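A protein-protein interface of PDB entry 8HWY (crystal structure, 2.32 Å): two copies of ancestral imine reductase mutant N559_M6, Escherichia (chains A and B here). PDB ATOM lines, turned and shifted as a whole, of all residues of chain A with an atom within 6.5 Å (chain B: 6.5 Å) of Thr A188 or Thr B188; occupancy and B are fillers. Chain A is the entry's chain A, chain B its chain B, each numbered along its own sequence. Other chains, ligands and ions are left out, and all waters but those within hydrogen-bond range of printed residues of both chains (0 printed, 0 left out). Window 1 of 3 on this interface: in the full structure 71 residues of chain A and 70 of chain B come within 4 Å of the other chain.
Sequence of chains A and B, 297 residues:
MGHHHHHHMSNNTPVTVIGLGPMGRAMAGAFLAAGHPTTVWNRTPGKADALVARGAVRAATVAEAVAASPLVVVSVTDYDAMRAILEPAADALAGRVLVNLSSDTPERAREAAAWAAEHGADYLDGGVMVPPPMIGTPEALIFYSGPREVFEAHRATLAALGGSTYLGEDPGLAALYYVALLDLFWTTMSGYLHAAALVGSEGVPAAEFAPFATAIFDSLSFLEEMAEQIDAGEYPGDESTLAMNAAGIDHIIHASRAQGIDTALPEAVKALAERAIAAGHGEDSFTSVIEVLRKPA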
ATOM      1  N   ASP A 183      14.413   6.388  10.952  1.00  0.00           N
ATOM      2  CA  ASP A 183      14.901   6.553   9.569  1.00  0.00           C
ATOM      3  C   ASP A 183      14.283   5.462   8.688  1.00  0.00           C
ATOM      4  O   ASP A 183      13.659   5.812   7.687  1.00  0.00           O
ATOM      5  CB  ASP A 183      16.425   6.574   9.571  1.00  0.00           C
ATOM      6  CG  ASP A 183      17.034   6.889   8.229  1.00  0.00           C
ATOM      7  OD1 ASP A 183      16.934   8.047   7.816  1.00  0.00           O
ATOM      8  OD2 ASP A 183      17.593   5.969   7.623  1.00  0.00           O
ATOM      9  N   LEU A 184      14.421   4.202   9.097  1.00  0.00           N
ATOM     10  CA  LEU A 184      13.880   3.096   8.317  1.00  0.00           C
ATOM     11  C   LEU A 184      12.374   3.240   8.128  1.00  0.00           C
ATOM     12  O   LEU A 184      11.843   2.965   7.044  1.00  0.00           O
ATOM     13  CB  LEU A 184      14.213   1.770   9.003  1.00  0.00           C
ATOM     14  CG  LEU A 184      13.601   0.519   8.360  1.00  0.00           C
ATOM     15  CD1 LEU A 184      13.860   0.441   6.831  1.00  0.00           C
ATOM     16  CD2 LEU A 184      14.166  -0.705   9.011  1.00  0.00           C
ATOM     17  N   PHE A 185      11.671   3.693   9.159  1.00  0.00           N
ATOM     18  CA  PHE A 185      10.215   3.717   9.093  1.00  0.00           C
ATOM     19  C   PHE A 185       9.721   4.718   8.057  1.00  0.00           C
ATOM     20  O   PHE A 185       8.962   4.366   7.150  1.00  0.00           O
ATOM     21  CB  PHE A 185       9.650   4.041  10.474  1.00  0.00           C
ATOM     22  CG  PHE A 185       8.162   4.084  10.519  1.00  0.00           C
ATOM     23  CD1 PHE A 185       7.437   2.925  10.673  1.00  0.00           C
ATOM     24  CD2 PHE A 185       7.478   5.294  10.411  1.00  0.00           C
ATOM     25  CE1 PHE A 185       6.043   2.968  10.736  1.00  0.00           C
ATOM     26  CE2 PHE A 185       6.093   5.345  10.470  1.00  0.00           C
ATOM     27  CZ  PHE A 185       5.374   4.177  10.622  1.00  0.00           C
ATOM     28  N   TRP A 186      10.133   5.987   8.183  1.00  0.00           N
ATOM     29  CA  TRP A 186       9.623   7.029   7.292  1.00  0.00           C
ATOM     30  C   TRP A 186      10.083   6.825   5.857  1.00  0.00           C
ATOM     31  O   TRP A 186       9.343   7.139   4.917  1.00  0.00           O
ATOM     32  CB  TRP A 186      10.043   8.415   7.790  1.00  0.00           C
ATOM     33  CG  TRP A 186       9.322   8.813   9.044  1.00  0.00           C
ATOM     34  CD1 TRP A 186       9.891   9.206  10.239  1.00  0.00           C
ATOM     35  CD2 TRP A 186       7.889   8.862   9.242  1.00  0.00           C
ATOM     36  NE1 TRP A 186       8.896   9.476  11.161  1.00  0.00           N
ATOM     37  CE2 TRP A 186       7.664   9.276  10.578  1.00  0.00           C
ATOM     38  CE3 TRP A 186       6.778   8.602   8.417  1.00  0.00           C
ATOM     39  CZ2 TRP A 186       6.366   9.423  11.114  1.00  0.00           C
ATOM     40  CZ3 TRP A 186       5.490   8.739   8.949  1.00  0.00           C
ATOM     41  CH2 TRP A 186       5.297   9.151  10.282  1.00  0.00           C
ATOM     42  N   THR A 187      11.285   6.283   5.660  1.00  0.00           N
ATOM     43  CA  THR A 187      11.703   5.952   4.310  1.00  0.00           C
ATOM     44  C   THR A 187      10.815   4.855   3.749  1.00  0.00           C
ATOM     45  O   THR A 187      10.341   4.935   2.609  1.00  0.00           O
ATOM     46  CB  THR A 187      13.167   5.517   4.310  1.00  0.00           C
ATOM     47  OG1 THR A 187      13.970   6.533   4.910  1.00  0.00           O
ATOM     48  CG2 THR A 187      13.664   5.308   2.918  1.00  0.00           C
ATOM     49  N   THR A 188      10.571   3.819   4.550  1.00  0.00           N
ATOM     50  CA  THR A 188       9.653   2.767   4.131  1.00  0.00           C
ATOM     51  C   THR A 188       8.288   3.345   3.796  1.00  0.00           C
ATOM     52  O   THR A 188       7.742   3.091   2.720  1.00  0.00           O
ATOM     53  CB  THR A 188       9.516   1.716   5.225  1.00  0.00           C
ATOM     54  OG1 THR A 188      10.820   1.191   5.513  1.00  0.00           O
ATOM     55  CG2 THR A 188       8.549   0.592   4.786  1.00  0.00           C
ATOM     56  N   MET A 189       7.714   4.121   4.717  1.00  0.00           N
ATOM     57  CA  MET A 189       6.418   4.750   4.453  1.00  0.00           C
ATOM     58  C   MET A 189       6.442   5.594   3.174  1.00  0.00           C
ATOM     59  O   MET A 189       5.466   5.617   2.409  1.00  0.00           O
ATOM     60  CB  MET A 189       6.021   5.598   5.659  1.00  0.00           C
ATOM     61  CG  MET A 189       4.580   5.437   6.072  1.00  0.00           C
ATOM     62  SD  MET A 189       4.422   3.771   6.750  1.00  0.00           S
ATOM     63  CE  MET A 189       3.820   2.931   5.293  1.00  0.00           C
ATOM     64  N   SER A 190       7.530   6.322   2.930  1.00  0.00           N
ATOM     65  CA  SER A 190       7.564   7.120   1.709  1.00  0.00           C
ATOM     66  C   SER A 190       7.618   6.226   0.479  1.00  0.00           C
ATOM     67  O   SER A 190       6.998   6.532  -0.546  1.00  0.00           O
ATOM     68  CB  SER A 190       8.751   8.078   1.734  1.00  0.00           C
ATOM     69  OG  SER A 190       8.821   8.737   2.987  1.00  0.00           O
ATOM     70  N   GLY A 191       8.367   5.130   0.547  1.00  0.00           N
ATOM     71  CA  GLY A 191       8.367   4.211  -0.574  1.00  0.00           C
ATOM     72  C   GLY A 191       6.974   3.681  -0.846  1.00  0.00           C
ATOM     73  O   GLY A 191       6.538   3.589  -1.998  1.00  0.00           O
ATOM     74  N   TYR A 192       6.238   3.372   0.216  1.00  0.00           N
ATOM     75  CA  TYR A 192       4.893   2.853   0.032  1.00  0.00           C
ATOM     76  C   TYR A 192       4.016   3.854  -0.700  1.00  0.00           C
ATOM     77  O   TYR A 192       3.323   3.503  -1.659  1.00  0.00           O
ATOM     78  CB  TYR A 192       4.284   2.513   1.370  1.00  0.00           C
ATOM     79  CG  TYR A 192       2.854   2.067   1.287  1.00  0.00           C
ATOM     80  CD1 TYR A 192       2.480   0.977   0.486  1.00  0.00           C
ATOM     81  CD2 TYR A 192       1.881   2.698   2.055  1.00  0.00           C
ATOM     82  CE1 TYR A 192       1.169   0.545   0.447  1.00  0.00           C
ATOM     83  CE2 TYR A 192       0.566   2.276   2.027  1.00  0.00           C
ATOM     84  CZ  TYR A 192       0.214   1.195   1.228  1.00  0.00           C
ATOM     85  OH  TYR A 192      -1.098   0.777   1.209  1.00  0.00           O
ATOM     86  N   LEU A 193       4.056   5.117  -0.271  1.00  0.00           N
ATOM     87  CA  LEU A 193       3.157   6.117  -0.837  1.00  0.00           C
ATOM     88  C   LEU A 193       3.523   6.419  -2.272  1.00  0.00           C
ATOM     89  O   LEU A 193       2.640   6.672  -3.096  1.00  0.00           O
ATOM     90  CB  LEU A 193       3.195   7.401  -0.024  1.00  0.00           C
ATOM     91  CG  LEU A 193       2.492   7.341   1.329  1.00  0.00           C
ATOM     92  CD1 LEU A 193       2.829   8.606   2.165  1.00  0.00           C
ATOM     93  CD2 LEU A 193       0.991   7.159   1.195  1.00  0.00           C
ATOM     94  N   ILE A 216       5.300  -8.133   0.143  1.00  0.00           N
ATOM     95  CA  ILE A 216       6.729  -7.877  -0.050  1.00  0.00           C
ATOM     96  C   ILE A 216       7.484  -8.078   1.248  1.00  0.00           C
ATOM     97  O   ILE A 216       8.644  -8.502   1.250  1.00  0.00           O
ATOM     98  CB  ILE A 216       6.944  -6.452  -0.616  1.00  0.00           C
ATOM     99  CG1 ILE A 216       7.113  -6.508  -2.130  1.00  0.00           C
ATOM    100  CG2 ILE A 216       8.161  -5.810  -0.029  1.00  0.00           C
ATOM    101  CD1 ILE A 216       6.008  -7.269  -2.823  1.00  0.00           C
ATOM    102  N   PHE A 217       6.833  -7.803   2.371  1.00  0.00           N
ATOM    103  CA  PHE A 217       7.487  -7.742   3.664  1.00  0.00           C
ATOM    104  C   PHE A 217       7.274  -8.998   4.507  1.00  0.00           C
ATOM    105  O   PHE A 217       7.434  -8.944   5.731  1.00  0.00           O
ATOM    106  CB  PHE A 217       6.981  -6.513   4.410  1.00  0.00           C
ATOM    107  CG  PHE A 217       7.308  -5.222   3.728  1.00  0.00           C
ATOM    108  CD1 PHE A 217       8.486  -5.095   2.985  1.00  0.00           C
ATOM    109  CD2 PHE A 217       6.451  -4.126   3.851  1.00  0.00           C
ATOM    110  CE1 PHE A 217       8.799  -3.897   2.360  1.00  0.00           C
ATOM    111  CE2 PHE A 217       6.749  -2.930   3.250  1.00  0.00           C
ATOM    112  CZ  PHE A 217       7.925  -2.808   2.499  1.00  0.00           C
ATOM    113  N   PHE A 222      15.782 -10.516   3.982  1.00  0.00           N
ATOM    114  CA  PHE A 222      16.811  -9.546   3.627  1.00  0.00           C
ATOM    115  C   PHE A 222      17.507  -8.964   4.860  1.00  0.00           C
ATOM    116  O   PHE A 222      18.699  -8.638   4.800  1.00  0.00           O
ATOM    117  CB  PHE A 222      16.184  -8.431   2.788  1.00  0.00           C
ATOM    118  CG  PHE A 222      15.162  -7.620   3.545  1.00  0.00           C
ATOM    119  CD1 PHE A 222      13.831  -8.052   3.628  1.00  0.00           C
ATOM    120  CD2 PHE A 222      15.543  -6.450   4.218  1.00  0.00           C
ATOM    121  CE1 PHE A 222      12.879  -7.314   4.347  1.00  0.00           C
ATOM    122  CE2 PHE A 222      14.613  -5.696   4.937  1.00  0.00           C
ATOM    123  CZ  PHE A 222      13.271  -6.124   5.004  1.00  0.00           C
ATOM    124  N   ASP B 183       9.760  -0.351  -6.543  1.00  0.00           N
ATOM    125  CA  ASP B 183       9.926   0.962  -5.942  1.00  0.00           C
ATOM    126  C   ASP B 183       9.828   0.889  -4.427  1.00  0.00           C
ATOM    127  O   ASP B 183      10.645   1.471  -3.708  1.00  0.00           O
ATOM    128  CB  ASP B 183       8.864   1.898  -6.513  1.00  0.00           C
ATOM    129  CG  ASP B 183       8.987   3.311  -5.987  1.00  0.00           C
ATOM    130  OD1 ASP B 183      10.140   3.707  -5.678  1.00  0.00           O
ATOM    131  OD2 ASP B 183       7.939   4.012  -5.887  1.00  0.00           O
ATOM    132  N   LEU B 184       8.818   0.187  -3.921  1.00  0.00           N
ATOM    133  CA  LEU B 184       8.717  -0.017  -2.482  1.00  0.00           C
ATOM    134  C   LEU B 184       9.899  -0.816  -1.956  1.00  0.00           C
ATOM    135  O   LEU B 184      10.421  -0.522  -0.874  1.00  0.00           O
ATOM    136  CB  LEU B 184       7.419  -0.736  -2.152  1.00  0.00           C
ATOM    137  CG  LEU B 184       7.165  -1.161  -0.709  1.00  0.00           C
ATOM    138  CD1 LEU B 184       7.464   0.000   0.260  1.00  0.00           C
ATOM    139  CD2 LEU B 184       5.702  -1.644  -0.547  1.00  0.00           C
ATOM    140  N   PHE B 185      10.346  -1.822  -2.709  1.00  0.00           N
ATOM    141  CA  PHE B 185      11.427  -2.682  -2.234  1.00  0.00           C
ATOM    142  C   PHE B 185      12.755  -1.937  -2.104  1.00  0.00           C
ATOM    143  O   PHE B 185      13.371  -1.936  -1.031  1.00  0.00           O
ATOM    144  CB  PHE B 185      11.608  -3.865  -3.163  1.00  0.00           C
ATOM    145  CG  PHE B 185      12.618  -4.829  -2.678  1.00  0.00           C
ATOM    146  CD1 PHE B 185      12.327  -5.687  -1.628  1.00  0.00           C
ATOM    147  CD2 PHE B 185      13.862  -4.883  -3.262  1.00  0.00           C
ATOM    148  CE1 PHE B 185      13.290  -6.593  -1.177  1.00  0.00           C
ATOM    149  CE2 PHE B 185      14.805  -5.782  -2.829  1.00  0.00           C
ATOM    150  CZ  PHE B 185      14.528  -6.634  -1.789  1.00  0.00           C
ATOM    151  N   TRP B 186      13.254  -1.353  -3.199  1.00  0.00           N
ATOM    152  CA  TRP B 186      14.563  -0.693  -3.141  1.00  0.00           C
ATOM    153  C   TRP B 186      14.557   0.532  -2.233  1.00  0.00           C
ATOM    154  O   TRP B 186      15.608   0.908  -1.696  1.00  0.00           O
ATOM    155  CB  TRP B 186      15.018  -0.296  -4.542  1.00  0.00           C
ATOM    156  CG  TRP B 186      15.230  -1.475  -5.382  1.00  0.00           C
ATOM    157  CD1 TRP B 186      14.586  -1.796  -6.556  1.00  0.00           C
ATOM    158  CD2 TRP B 186      16.141  -2.536  -5.117  1.00  0.00           C
ATOM    159  NE1 TRP B 186      15.054  -3.003  -7.029  1.00  0.00           N
ATOM    160  CE2 TRP B 186      16.013  -3.477  -6.169  1.00  0.00           C
ATOM    161  CE3 TRP B 186      17.067  -2.782  -4.100  1.00  0.00           C
ATOM    162  CZ2 TRP B 186      16.783  -4.645  -6.229  1.00  0.00           C
ATOM    163  CZ3 TRP B 186      17.833  -3.951  -4.161  1.00  0.00           C
ATOM    164  CH2 TRP B 186      17.679  -4.866  -5.220  1.00  0.00           C
ATOM    165  N   THR B 187      13.402   1.177  -2.063  1.00  0.00           N
ATOM    166  CA  THR B 187      13.345   2.324  -1.171  1.00  0.00           C
ATOM    167  C   THR B 187      13.460   1.877   0.264  1.00  0.00           C
ATOM    168  O   THR B 187      14.157   2.510   1.063  1.00  0.00           O
ATOM    169  CB  THR B 187      12.063   3.109  -1.390  1.00  0.00           C
ATOM    170  OG1 THR B 187      12.082   3.586  -2.731  1.00  0.00           O
ATOM    171  CG2 THR B 187      11.988   4.317  -0.434  1.00  0.00           C
ATOM    172  N   THR B 188      12.842   0.739   0.580  1.00  0.00           N
ATOM    173  CA  THR B 188      12.955   0.177   1.917  1.00  0.00           C
ATOM    174  C   THR B 188      14.367  -0.307   2.193  1.00  0.00           C
ATOM    175  O   THR B 188      14.936   0.000   3.242  1.00  0.00           O
ATOM    176  CB  THR B 188      11.967  -0.967   2.118  1.00  0.00           C
ATOM    177  OG1 THR B 188      10.628  -0.485   1.916  1.00  0.00           O
ATOM    178  CG2 THR B 188      12.134  -1.523   3.556  1.00  0.00           C
ATOM    179  N   MET B 189      14.950  -1.077   1.276  1.00  0.00           N
ATOM    180  CA  MET B 189      16.344  -1.475   1.434  1.00  0.00           C
ATOM    181  C   MET B 189      17.245  -0.276   1.728  1.00  0.00           C
ATOM    182  O   MET B 189      18.088  -0.323   2.631  1.00  0.00           O
ATOM    183  CB  MET B 189      16.819  -2.196   0.174  1.00  0.00           C
ATOM    184  CG  MET B 189      16.000  -3.446  -0.156  1.00  0.00           C
ATOM    185  SD  MET B 189      16.042  -4.634   1.216  1.00  0.00           S
ATOM    186  CE  MET B 189      14.298  -4.727   1.685  1.00  0.00           C
ATOM    187  N   SER B 190      17.109   0.798   0.950  1.00  0.00           N
ATOM    188  CA  SER B 190      17.972   1.956   1.163  1.00  0.00           C
ATOM    189  C   SER B 190      17.766   2.533   2.554  1.00  0.00           C
ATOM    190  O   SER B 190      18.730   2.811   3.275  1.00  0.00           O
ATOM    191  CB  SER B 190      17.714   3.011   0.091  1.00  0.00           C
ATOM    192  OG  SER B 190      17.919   2.440  -1.187  1.00  0.00           O
ATOM    193  N   GLY B 191      16.509   2.683   2.967  1.00  0.00           N
ATOM    194  CA  GLY B 191      16.262   3.122   4.324  1.00  0.00           C
ATOM    195  C   GLY B 191      16.925   2.204   5.321  1.00  0.00           C
ATOM    196  O   GLY B 191      17.562   2.654   6.280  1.00  0.00           O
ATOM    197  N   TYR B 192      16.847   0.899   5.074  1.00  0.00           N
ATOM    198  CA  TYR B 192      17.435  -0.021   6.029  1.00  0.00           C
ATOM    199  C   TYR B 192      18.942   0.156   6.096  1.00  0.00           C
ATOM    200  O   TYR B 192      19.529   0.103   7.180  1.00  0.00           O
ATOM    201  CB  TYR B 192      17.090  -1.447   5.670  1.00  0.00           C
ATOM    202  CG  TYR B 192      17.787  -2.448   6.534  1.00  0.00           C
ATOM    203  CD1 TYR B 192      17.522  -2.535   7.893  1.00  0.00           C
ATOM    204  CD2 TYR B 192      18.715  -3.314   5.987  1.00  0.00           C
ATOM    205  CE1 TYR B 192      18.155  -3.490   8.690  1.00  0.00           C
ATOM    206  CE2 TYR B 192      19.355  -4.274   6.767  1.00  0.00           C
ATOM    207  CZ  TYR B 192      19.072  -4.365   8.115  1.00  0.00           C
ATOM    208  OH  TYR B 192      19.714  -5.333   8.867  1.00  0.00           O
ATOM    209  N   LEU B 193      19.580   0.403   4.956  1.00  0.00           N
ATOM    210  CA  LEU B 193      21.025   0.587   4.966  1.00  0.00           C
ATOM    211  C   LEU B 193      21.397   1.904   5.629  1.00  0.00           C
ATOM    212  O   LEU B 193      22.394   1.981   6.362  1.00  0.00           O
ATOM    213  CB  LEU B 193      21.558   0.522   3.537  1.00  0.00           C
ATOM    214  CG  LEU B 193      21.393  -0.854   2.888  1.00  0.00           C
ATOM    215  CD1 LEU B 193      21.961  -0.844   1.462  1.00  0.00           C
ATOM    216  CD2 LEU B 193      22.051  -1.962   3.774  1.00  0.00           C
ATOM    217  N   ILE B 216       9.844  -3.243  13.262  1.00  0.00           N
ATOM    218  CA  ILE B 216       9.161  -2.203  12.490  1.00  0.00           C
ATOM    219  C   ILE B 216       8.083  -2.836  11.625  1.00  0.00           C
ATOM    220  O   ILE B 216       6.895  -2.529  11.753  1.00  0.00           O
ATOM    221  CB  ILE B 216      10.162  -1.409  11.634  1.00  0.00           C
ATOM    222  CG1 ILE B 216      10.892  -0.360  12.472  1.00  0.00           C
ATOM    223  CG2 ILE B 216       9.473  -0.757  10.460  1.00  0.00           C
ATOM    224  CD1 ILE B 216      12.108   0.279  11.733  1.00  0.00           C
ATOM    225  N   PHE B 217       8.488  -3.738  10.737  1.00  0.00           N
ATOM    226  CA  PHE B 217       7.539  -4.619  10.081  1.00  0.00           C
ATOM    227  C   PHE B 217       6.920  -5.572  11.101  1.00  0.00           C
ATOM    228  O   PHE B 217       7.406  -5.716  12.225  1.00  0.00           O
ATOM    229  CB  PHE B 217       8.233  -5.401   8.985  1.00  0.00           C
ATOM    230  CG  PHE B 217       9.326  -4.641   8.317  1.00  0.00           C
ATOM    231  CD1 PHE B 217       9.045  -3.748   7.304  1.00  0.00           C
ATOM    232  CD2 PHE B 217      10.640  -4.817   8.697  1.00  0.00           C
ATOM    233  CE1 PHE B 217      10.073  -3.048   6.663  1.00  0.00           C
ATOM    234  CE2 PHE B 217      11.666  -4.132   8.065  1.00  0.00           C
ATOM    235  CZ  PHE B 217      11.381  -3.242   7.042  1.00  0.00           C
ATOM    236  N   LEU B 223      -0.383  -0.459   6.555  1.00  0.00           N
ATOM    237  CA  LEU B 223      -0.485  -0.223   5.116  1.00  0.00           C
ATOM    238  C   LEU B 223      -1.935  -0.195   4.656  1.00  0.00           C
ATOM    239  O   LEU B 223      -2.349   0.697   3.904  1.00  0.00           O
ATOM    240  CB  LEU B 223       0.289  -1.290   4.346  1.00  0.00           C
ATOM    241  CG  LEU B 223       1.788  -1.229   4.622  1.00  0.00           C
ATOM    242  CD1 LEU B 223       2.582  -1.612   3.376  1.00  0.00           C
ATOM    243  CD2 LEU B 223       2.224   0.151   5.132  1.00  0.00           C
ATOM    244  N   VAL B 269      13.368  12.342   1.899  1.00  0.00           N
ATOM    245  CA  VAL B 269      12.116  12.150   2.619  1.00  0.00           C
ATOM    246  C   VAL B 269      11.621  13.480   3.177  1.00  0.00           C
ATOM    247  O   VAL B 269      10.447  13.845   3.008  1.00  0.00           O
ATOM    248  CB  VAL B 269      12.313  11.094   3.717  1.00  0.00           C
ATOM    249  CG1 VAL B 269      11.088  10.998   4.583  1.00  0.00           C
ATOM    250  CG2 VAL B 269      12.701   9.740   3.071  1.00  0.00           C
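Of the 14 printed residues of chain A, 10 touch a printed residue of chain B. Printed residues of chain A that touch a printed residue of chain B: Asp A183, Leu A184, Thr A187, Thr A188, Met A189, Ser A190, Gly A191, Tyr A192, Phe A217 and Phe A222. Printed residues of chain B that touch a printed residue of chain A: Leu B184, Thr B187, Thr B188, Met B189, Gly B191, Tyr B192, Ile B216, Phe B217, Leu B223 and Val B269. Among the printed residues, 20 pairs touch across the chains. Among the printed residues, no Asp or Glu carboxylate lies within 4 Å of a Lys or Arg side-chain nitrogen of the other chain.
The backbone carbonyl oxygen (O) of Leu B223 lies within hydrogen-bond range of the side-chain hydroxyl (OH) of Tyr A192 (3.0 Å).
O of Asp A183 lies within hydrogen-bond range of OG1 of Thr A187. The backbone carbonyl oxygen (O) of Leu B184 lies within hydrogen-bond range of the side-chain hydroxyl (OG1) of Thr B188, at 2.8 Å. The backbone carbonyl oxygen (O) of Trp A186 lies within hydrogen-bond range of the side-chain hydroxyl (OG) of Ser A190. The backbone carbonyl oxygen (O) of Asp B183 sits at hydrogen-bond distance from the side-chain hydroxyl (OG1) of Thr B187 (2.7 Å). The backbone carbonyl oxygen (O) of Leu A184 is in hydrogen-bond range of the side-chain hydroxyl (OG1) of Thr A188, 2.6 Å away.
Thr A188 touches just these residues of chain B: Leu B184 (3.96 Å) and Thr B188 (3.6 Å). Printed residues of chain B within 4 Å of Gly A191: Leu B184 (3.9 Å) and Thr B187 (3.6 Å). Of the printed residues of chain A, Leu B184 touches Thr A188 (3.96 Å), Gly A191 (3.9 Å), Tyr A192 (3.6 Å) and Phe A217 (3.6 Å). Of chain A, only Leu A184, Thr A188 and Phe A217 come within 4 Å of Thr B188. Of the printed residues of chain A, Ile B216 touches Leu A184. The nearest residue of chain A that does not touch Thr B188 is Phe A222 (5.0 Å). The nearest printed residue of chain B that does not touch Gly A191 is Asp B183 (4.2 Å).
Leu A184 touches Tyr B192, and with the chains exchanged Tyr A192 touches Leu B184. Thr A187 touches its own counterpart, Thr B187. Thr A188 touches its own counterpart, Thr B188. Phe A217 touches Thr B188, but with the chains exchanged Thr A188 does not touch Phe B217 (4.4 Å). 13 positions are printed for both chains.
Asp A183 touches Gly B191 (OD2 to O, 3.6 Å). Leu A184 touches Thr B188 (CD1 to O, 3.8 Å). Thr A187 touches Thr B187 (CG2 to O, 3.4 Å). Ser A190 touches Val B269 (OG to CG1, 3.6 Å). Leu B184 touches Gly A191 (CD1 to C, 3.9 Å). Thr B187 touches Gly A191 (CG2 to CA, 3.6 Å). CZ of Phe A217 touches CD1 of Leu B184 (3.6 Å). Phe A217 touches Thr B188. Phe A222 touches Met B189. Phe A222 touches Phe B217 (CZ to CE2, 3.99 Å).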
